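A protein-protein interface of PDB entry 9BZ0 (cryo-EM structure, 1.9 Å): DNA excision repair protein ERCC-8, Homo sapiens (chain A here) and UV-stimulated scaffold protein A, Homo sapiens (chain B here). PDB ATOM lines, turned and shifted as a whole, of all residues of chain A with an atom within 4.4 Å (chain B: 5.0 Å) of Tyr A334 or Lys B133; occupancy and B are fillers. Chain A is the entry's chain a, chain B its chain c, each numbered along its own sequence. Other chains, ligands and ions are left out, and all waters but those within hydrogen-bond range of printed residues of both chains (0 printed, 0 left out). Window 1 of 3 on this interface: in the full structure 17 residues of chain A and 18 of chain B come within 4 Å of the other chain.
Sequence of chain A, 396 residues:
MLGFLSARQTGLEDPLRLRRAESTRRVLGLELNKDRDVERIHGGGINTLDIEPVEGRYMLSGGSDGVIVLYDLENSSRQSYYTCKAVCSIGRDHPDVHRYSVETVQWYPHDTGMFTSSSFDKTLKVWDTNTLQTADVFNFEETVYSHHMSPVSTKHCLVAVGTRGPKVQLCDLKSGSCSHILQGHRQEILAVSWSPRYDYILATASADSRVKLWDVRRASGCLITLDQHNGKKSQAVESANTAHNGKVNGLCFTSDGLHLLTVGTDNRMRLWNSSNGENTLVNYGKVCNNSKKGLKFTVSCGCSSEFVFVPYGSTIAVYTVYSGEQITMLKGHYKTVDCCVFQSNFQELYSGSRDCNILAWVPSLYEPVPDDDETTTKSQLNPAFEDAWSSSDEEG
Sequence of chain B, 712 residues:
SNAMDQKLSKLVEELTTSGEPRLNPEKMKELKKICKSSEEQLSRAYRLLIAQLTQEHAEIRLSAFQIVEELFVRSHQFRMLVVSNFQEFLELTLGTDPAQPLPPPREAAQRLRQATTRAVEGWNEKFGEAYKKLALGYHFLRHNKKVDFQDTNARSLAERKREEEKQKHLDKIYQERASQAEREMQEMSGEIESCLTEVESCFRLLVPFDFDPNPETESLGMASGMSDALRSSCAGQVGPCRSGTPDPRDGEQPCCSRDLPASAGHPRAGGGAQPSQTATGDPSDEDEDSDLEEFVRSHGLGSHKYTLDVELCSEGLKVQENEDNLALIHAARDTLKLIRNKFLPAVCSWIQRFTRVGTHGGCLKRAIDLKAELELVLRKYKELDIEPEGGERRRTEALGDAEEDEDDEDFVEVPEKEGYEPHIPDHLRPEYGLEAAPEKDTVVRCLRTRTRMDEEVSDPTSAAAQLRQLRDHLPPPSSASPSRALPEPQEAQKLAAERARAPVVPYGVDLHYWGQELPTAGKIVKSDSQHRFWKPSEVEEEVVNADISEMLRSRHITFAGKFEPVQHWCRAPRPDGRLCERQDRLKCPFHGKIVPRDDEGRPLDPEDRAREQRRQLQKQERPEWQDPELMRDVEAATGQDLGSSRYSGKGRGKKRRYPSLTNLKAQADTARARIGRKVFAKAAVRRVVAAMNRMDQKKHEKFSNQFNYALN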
ATOM      1  N   LYS A 331      23.838 -26.489 -18.302  1.00  0.00           N
ATOM      2  CA  LYS A 331      22.535 -25.961 -17.916  1.00  0.00           C
ATOM      3  C   LYS A 331      21.458 -27.037 -17.732  1.00  0.00           C
ATOM      4  O   LYS A 331      20.306 -26.854 -18.124  1.00  0.00           O
ATOM      5  CB  LYS A 331      22.103 -24.897 -18.916  1.00  0.00           C
ATOM      6  CG  LYS A 331      21.287 -23.802 -18.296  1.00  0.00           C
ATOM      7  CD  LYS A 331      21.262 -22.581 -19.180  1.00  0.00           C
ATOM      8  CE  LYS A 331      20.419 -21.480 -18.568  1.00  0.00           C
ATOM      9  NZ  LYS A 331      20.482 -20.215 -19.352  1.00  0.00           N
ATOM     10  N   GLY A 332      21.821 -28.178 -17.158  1.00  0.00           N
ATOM     11  CA  GLY A 332      20.991 -29.372 -17.147  1.00  0.00           C
ATOM     12  C   GLY A 332      20.035 -29.580 -15.981  1.00  0.00           C
ATOM     13  O   GLY A 332      18.852 -29.836 -16.193  1.00  0.00           O
ATOM     14  N   HIS A 333      20.542 -29.513 -14.752  1.00  0.00           N
ATOM     15  CA  HIS A 333      19.809 -29.883 -13.546  1.00  0.00           C
ATOM     16  C   HIS A 333      18.655 -28.934 -13.235  1.00  0.00           C
ATOM     17  O   HIS A 333      18.619 -27.787 -13.679  1.00  0.00           O
ATOM     18  CB  HIS A 333      20.747 -29.909 -12.342  1.00  0.00           C
ATOM     19  CG  HIS A 333      21.702 -31.054 -12.340  1.00  0.00           C
ATOM     20  ND1 HIS A 333      21.317 -32.336 -12.029  1.00  0.00           N
ATOM     21  CD2 HIS A 333      23.023 -31.115 -12.613  1.00  0.00           C
ATOM     22  CE1 HIS A 333      22.361 -33.136 -12.105  1.00  0.00           C
ATOM     23  NE2 HIS A 333      23.409 -32.419 -12.456  1.00  0.00           N
ATOM     24  N   TYR A 334      17.699 -29.439 -12.448  1.00  0.00           N
ATOM     25  CA  TYR A 334      16.519 -28.685 -12.039  1.00  0.00           C
ATOM     26  C   TYR A 334      16.573 -28.170 -10.608  1.00  0.00           C
ATOM     27  O   TYR A 334      15.710 -27.379 -10.223  1.00  0.00           O
ATOM     28  CB  TYR A 334      15.254 -29.513 -12.231  1.00  0.00           C
ATOM     29  CG  TYR A 334      14.878 -29.557 -13.667  1.00  0.00           C
ATOM     30  CD1 TYR A 334      14.095 -28.573 -14.219  1.00  0.00           C
ATOM     31  CD2 TYR A 334      15.330 -30.562 -14.484  1.00  0.00           C
ATOM     32  CE1 TYR A 334      13.747 -28.608 -15.530  1.00  0.00           C
ATOM     33  CE2 TYR A 334      15.004 -30.592 -15.802  1.00  0.00           C
ATOM     34  CZ  TYR A 334      14.212 -29.611 -16.320  1.00  0.00           C
ATOM     35  OH  TYR A 334      13.895 -29.622 -17.653  1.00  0.00           O
ATOM     36  N   LYS A 335      17.559 -28.578  -9.824  1.00  0.00           N
ATOM     37  CA  LYS A 335      17.751 -28.079  -8.474  1.00  0.00           C
ATOM     38  C   LYS A 335      19.236 -27.852  -8.271  1.00  0.00           C
ATOM     39  O   LYS A 335      20.048 -28.203  -9.126  1.00  0.00           O
ATOM     40  CB  LYS A 335      17.180 -29.024  -7.422  1.00  0.00           C
ATOM     41  CG  LYS A 335      15.676 -29.062  -7.386  1.00  0.00           C
ATOM     42  CD  LYS A 335      15.188 -29.887  -6.224  1.00  0.00           C
ATOM     43  CE  LYS A 335      13.696 -29.742  -6.033  1.00  0.00           C
ATOM     44  NZ  LYS A 335      13.212 -30.531  -4.869  1.00  0.00           N
ATOM     45  N   ASP A 355      17.979 -32.656  -7.454  1.00  0.00           N
ATOM     46  CA  ASP A 355      16.956 -33.182  -8.347  1.00  0.00           C
ATOM     47  C   ASP A 355      17.048 -34.687  -8.542  1.00  0.00           C
ATOM     48  O   ASP A 355      16.297 -35.232  -9.352  1.00  0.00           O
ATOM     49  CB  ASP A 355      17.000 -32.444  -9.689  1.00  0.00           C
ATOM     50  CG  ASP A 355      18.185 -32.827 -10.557  1.00  0.00           C
ATOM     51  OD1 ASP A 355      18.997 -33.694 -10.182  1.00  0.00           O
ATOM     52  OD2 ASP A 355      18.303 -32.245 -11.651  1.00  0.00           O
ATOM     53  N   VAL B  83      13.459 -24.701 -23.986  1.00  0.00           N
ATOM     54  CA  VAL B  83      14.043 -25.794 -23.217  1.00  0.00           C
ATOM     55  C   VAL B  83      15.314 -25.362 -22.501  1.00  0.00           C
ATOM     56  O   VAL B  83      15.627 -25.873 -21.419  1.00  0.00           O
ATOM     57  CB  VAL B  83      14.281 -27.002 -24.138  1.00  0.00           C
ATOM     58  CG1 VAL B  83      15.053 -28.082 -23.424  1.00  0.00           C
ATOM     59  CG2 VAL B  83      12.966 -27.558 -24.607  1.00  0.00           C
ATOM     60  N   SER B  84      16.048 -24.401 -23.057  1.00  0.00           N
ATOM     61  CA  SER B  84      17.248 -23.907 -22.389  1.00  0.00           C
ATOM     62  C   SER B  84      16.968 -23.252 -21.041  1.00  0.00           C
ATOM     63  O   SER B  84      17.906 -23.058 -20.263  1.00  0.00           O
ATOM     64  CB  SER B  84      17.975 -22.915 -23.293  1.00  0.00           C
ATOM     65  OG  SER B  84      17.350 -21.645 -23.250  1.00  0.00           O
ATOM     66  N   ASN B  85      15.717 -22.897 -20.743  1.00  0.00           N
ATOM     67  CA  ASN B  85      15.378 -22.273 -19.467  1.00  0.00           C
ATOM     68  C   ASN B  85      14.170 -22.948 -18.823  1.00  0.00           C
ATOM     69  O   ASN B  85      13.474 -22.350 -18.004  1.00  0.00           O
ATOM     70  CB  ASN B  85      15.137 -20.776 -19.650  1.00  0.00           C
ATOM     71  CG  ASN B  85      15.231 -20.008 -18.350  1.00  0.00           C
ATOM     72  OD1 ASN B  85      15.945 -20.406 -17.430  1.00  0.00           O
ATOM     73  ND2 ASN B  85      14.511 -18.895 -18.266  1.00  0.00           N
ATOM     74  N   PHE B  86      13.948 -24.213 -19.161  1.00  0.00           N
ATOM     75  CA  PHE B  86      12.722 -24.908 -18.801  1.00  0.00           C
ATOM     76  C   PHE B  86      12.480 -24.928 -17.302  1.00  0.00           C
ATOM     77  O   PHE B  86      11.330 -24.990 -16.863  1.00  0.00           O
ATOM     78  CB  PHE B  86      12.788 -26.334 -19.337  1.00  0.00           C
ATOM     79  CG  PHE B  86      11.466 -26.917 -19.687  1.00  0.00           C
ATOM     80  CD1 PHE B  86      10.708 -26.378 -20.696  1.00  0.00           C
ATOM     81  CD2 PHE B  86      11.008 -28.039 -19.042  1.00  0.00           C
ATOM     82  CE1 PHE B  86       9.499 -26.925 -21.027  1.00  0.00           C
ATOM     83  CE2 PHE B  86       9.803 -28.590 -19.369  1.00  0.00           C
ATOM     84  CZ  PHE B  86       9.047 -28.034 -20.364  1.00  0.00           C
ATOM     85  N   GLN B  87      13.541 -24.878 -16.500  1.00  0.00           N
ATOM     86  CA  GLN B  87      13.371 -24.819 -15.054  1.00  0.00           C
ATOM     87  C   GLN B  87      12.622 -23.559 -14.637  1.00  0.00           C
ATOM     88  O   GLN B  87      11.603 -23.624 -13.934  1.00  0.00           O
ATOM     89  CB  GLN B  87      14.740 -24.892 -14.382  1.00  0.00           C
ATOM     90  CG  GLN B  87      14.701 -24.960 -12.877  1.00  0.00           C
ATOM     91  CD  GLN B  87      15.884 -24.263 -12.247  1.00  0.00           C
ATOM     92  OE1 GLN B  87      17.015 -24.400 -12.710  1.00  0.00           O
ATOM     93  NE2 GLN B  87      15.632 -23.507 -11.187  1.00  0.00           N
ATOM     94  N   LEU B  90       8.939 -23.631 -16.025  1.00  0.00           N
ATOM     95  CA  LEU B  90       8.027 -24.400 -15.189  1.00  0.00           C
ATOM     96  C   LEU B  90       7.758 -23.718 -13.862  1.00  0.00           C
ATOM     97  O   LEU B  90       6.646 -23.819 -13.335  1.00  0.00           O
ATOM     98  CB  LEU B  90       8.578 -25.804 -14.961  1.00  0.00           C
ATOM     99  CG  LEU B  90       8.660 -26.690 -16.198  1.00  0.00           C
ATOM    100  CD1 LEU B  90       9.317 -28.006 -15.853  1.00  0.00           C
ATOM    101  CD2 LEU B  90       7.281 -26.917 -16.765  1.00  0.00           C
ATOM    102  N   TYR B 131      15.027 -33.629 -27.169  1.00  0.00           N
ATOM    103  CA  TYR B 131      15.451 -32.591 -26.229  1.00  0.00           C
ATOM    104  C   TYR B 131      15.602 -33.206 -24.840  1.00  0.00           C
ATOM    105  O   TYR B 131      14.644 -33.291 -24.073  1.00  0.00           O
ATOM    106  CB  TYR B 131      14.454 -31.444 -26.225  1.00  0.00           C
ATOM    107  CG  TYR B 131      14.375 -30.712 -27.541  1.00  0.00           C
ATOM    108  CD1 TYR B 131      13.548 -31.167 -28.555  1.00  0.00           C
ATOM    109  CD2 TYR B 131      15.133 -29.577 -27.775  1.00  0.00           C
ATOM    110  CE1 TYR B 131      13.473 -30.513 -29.757  1.00  0.00           C
ATOM    111  CE2 TYR B 131      15.060 -28.913 -28.979  1.00  0.00           C
ATOM    112  CZ  TYR B 131      14.231 -29.388 -29.965  1.00  0.00           C
ATOM    113  OH  TYR B 131      14.151 -28.724 -31.165  1.00  0.00           O
ATOM    114  N   LYS B 132      16.819 -33.662 -24.534  1.00  0.00           N
ATOM    115  CA  LYS B 132      17.086 -34.399 -23.300  1.00  0.00           C
ATOM    116  C   LYS B 132      16.566 -33.674 -22.067  1.00  0.00           C
ATOM    117  O   LYS B 132      15.974 -34.288 -21.167  1.00  0.00           O
ATOM    118  CB  LYS B 132      18.592 -34.613 -23.155  1.00  0.00           C
ATOM    119  CG  LYS B 132      19.239 -35.453 -24.232  1.00  0.00           C
ATOM    120  CD  LYS B 132      18.795 -36.891 -24.181  1.00  0.00           C
ATOM    121  CE  LYS B 132      19.495 -37.702 -25.254  1.00  0.00           C
ATOM    122  NZ  LYS B 132      19.058 -39.124 -25.241  1.00  0.00           N
ATOM    123  N   LYS B 133      16.769 -32.361 -22.016  1.00  0.00           N
ATOM    124  CA  LYS B 133      16.356 -31.590 -20.853  1.00  0.00           C
ATOM    125  C   LYS B 133      14.842 -31.540 -20.709  1.00  0.00           C
ATOM    126  O   LYS B 133      14.332 -31.444 -19.589  1.00  0.00           O
ATOM    127  CB  LYS B 133      16.964 -30.193 -20.935  1.00  0.00           C
ATOM    128  CG  LYS B 133      16.668 -29.298 -19.752  1.00  0.00           C
ATOM    129  CD  LYS B 133      17.491 -28.023 -19.824  1.00  0.00           C
ATOM    130  CE  LYS B 133      17.052 -27.012 -18.779  1.00  0.00           C
ATOM    131  NZ  LYS B 133      17.574 -27.341 -17.429  1.00  0.00           N
ATOM    132  N   LEU B 134      14.106 -31.696 -21.805  1.00  0.00           N
ATOM    133  CA  LEU B 134      12.654 -31.787 -21.707  1.00  0.00           C
ATOM    134  C   LEU B 134      12.208 -33.088 -21.051  1.00  0.00           C
ATOM    135  O   LEU B 134      11.295 -33.084 -20.216  1.00  0.00           O
ATOM    136  CB  LEU B 134      12.042 -31.646 -23.099  1.00  0.00           C
ATOM    137  CG  LEU B 134      10.533 -31.766 -23.273  1.00  0.00           C
ATOM    138  CD1 LEU B 134       9.813 -30.676 -22.520  1.00  0.00           C
ATOM    139  CD2 LEU B 134      10.193 -31.707 -24.742  1.00  0.00           C
ATOM    140  N   ALA B 135      12.824 -34.210 -21.410  1.00  0.00           N
ATOM    141  CA  ALA B 135      12.496 -35.467 -20.748  1.00  0.00           C
ATOM    142  C   ALA B 135      12.881 -35.456 -19.277  1.00  0.00           C
ATOM    143  O   ALA B 135      12.124 -35.948 -18.427  1.00  0.00           O
ATOM    144  CB  ALA B 135      13.180 -36.625 -21.464  1.00  0.00           C
ATOM    145  N   LEU B 136      14.033 -34.870 -18.947  1.00  0.00           N
ATOM    146  CA  LEU B 136      14.380 -34.690 -17.541  1.00  0.00           C
ATOM    147  C   LEU B 136      13.361 -33.830 -16.813  1.00  0.00           C
ATOM    148  O   LEU B 136      12.994 -34.127 -15.672  1.00  0.00           O
ATOM    149  CB  LEU B 136      15.772 -34.081 -17.413  1.00  0.00           C
ATOM    150  CG  LEU B 136      16.962 -34.908 -17.883  1.00  0.00           C
ATOM    151  CD1 LEU B 136      18.231 -34.106 -17.735  1.00  0.00           C
ATOM    152  CD2 LEU B 136      17.057 -36.182 -17.087  1.00  0.00           C
ATOM    153  N   GLY B 137      12.907 -32.753 -17.442  1.00  0.00           N
ATOM    154  CA  GLY B 137      11.906 -31.904 -16.820  1.00  0.00           C
ATOM    155  C   GLY B 137      10.598 -32.618 -16.564  1.00  0.00           C
ATOM    156  O   GLY B 137       9.992 -32.476 -15.498  1.00  0.00           O
ATOM    157  N   PHE B 140      11.109 -34.905 -13.620  1.00  0.00           N
ATOM    158  CA  PHE B 140      11.120 -34.076 -12.422  1.00  0.00           C
ATOM    159  C   PHE B 140       9.724 -33.690 -11.971  1.00  0.00           C
ATOM    160  O   PHE B 140       9.381 -33.839 -10.793  1.00  0.00           O
ATOM    161  CB  PHE B 140      11.953 -32.831 -12.695  1.00  0.00           C
ATOM    162  CG  PHE B 140      11.930 -31.827 -11.597  1.00  0.00           C
ATOM    163  CD1 PHE B 140      12.620 -32.039 -10.429  1.00  0.00           C
ATOM    164  CD2 PHE B 140      11.264 -30.635 -11.762  1.00  0.00           C
ATOM    165  CE1 PHE B 140      12.611 -31.096  -9.435  1.00  0.00           C
ATOM    166  CE2 PHE B 140      11.255 -29.696 -10.774  1.00  0.00           C
ATOM    167  CZ  PHE B 140      11.928 -29.925  -9.612  1.00  0.00           C
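Of chain B, only Phe B86 (3.6 Å), Gln B87 (3.7 Å), Lys B133 (2.7 Å), Leu B136 (3.8 Å) and Gly B137 (3.1 Å) come within 4 Å of Tyr A334. Printed residues of chain A within 4 Å of Lys B133: Lys A331, Gly A332, His A333 and Tyr A334. Of the printed residues of chain A, Gln B87 touches His A333 and Tyr A334. Printed residues of chain A within 4 Å of Gly B137: Tyr A334 (3.1 Å). Ala B135 touches none of the printed residues of chain A. The nearest residue of chain B that does not touch Tyr A334 is Phe B140 (4.1 Å). The nearest printed residue of chain B that does not touch His A333 is Leu B136 (5.9 Å).
ND1 of His A333 is in hydrogen-bond range of OD2 of Asp A355 (3.0 Å). OD2 of Asp A355 is in hydrogen-bond range of N of Tyr A334.
Among the printed residues, merely in contact across the chains: Lys A331 with Ser B84, Tyr A334 with Phe B86, Tyr A334 with Gln B87, Tyr A334 with Leu B136, Lys A335 with Phe B140, His A333 with Gln B87 and His A333 with Lys B133.
Of the 6 printed residues of chain A, 5 touch a printed residue of chain B. Printed residues of chain A that touch a printed residue of chain B: Lys A331, Gly A332, His A333, Tyr A334 and Lys A335. Hydrophobic or aromatic side chains of chain A within 4 Å of the printed part of chain B: Tyr A334. Among the printed residues, 11 pairs touch across the chains.
The backbone carbonyl oxygen (O) of Lys A331 lies within hydrogen-bond range of the side-chain amino group (NZ) of Lys B133 (2.9 Å). The backbone carbonyl oxygen (O) of Gly A332 lies within hydrogen-bond range of the side-chain amino group (NZ) of Lys B133. The side-chain hydroxyl of Tyr A334 sits at hydrogen-bond distance from the backbone carbonyl oxygen of Lys B133. The backbone NH (N) of Gly B137 lies close to the side-chain hydroxyl (OH) of Tyr A334.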
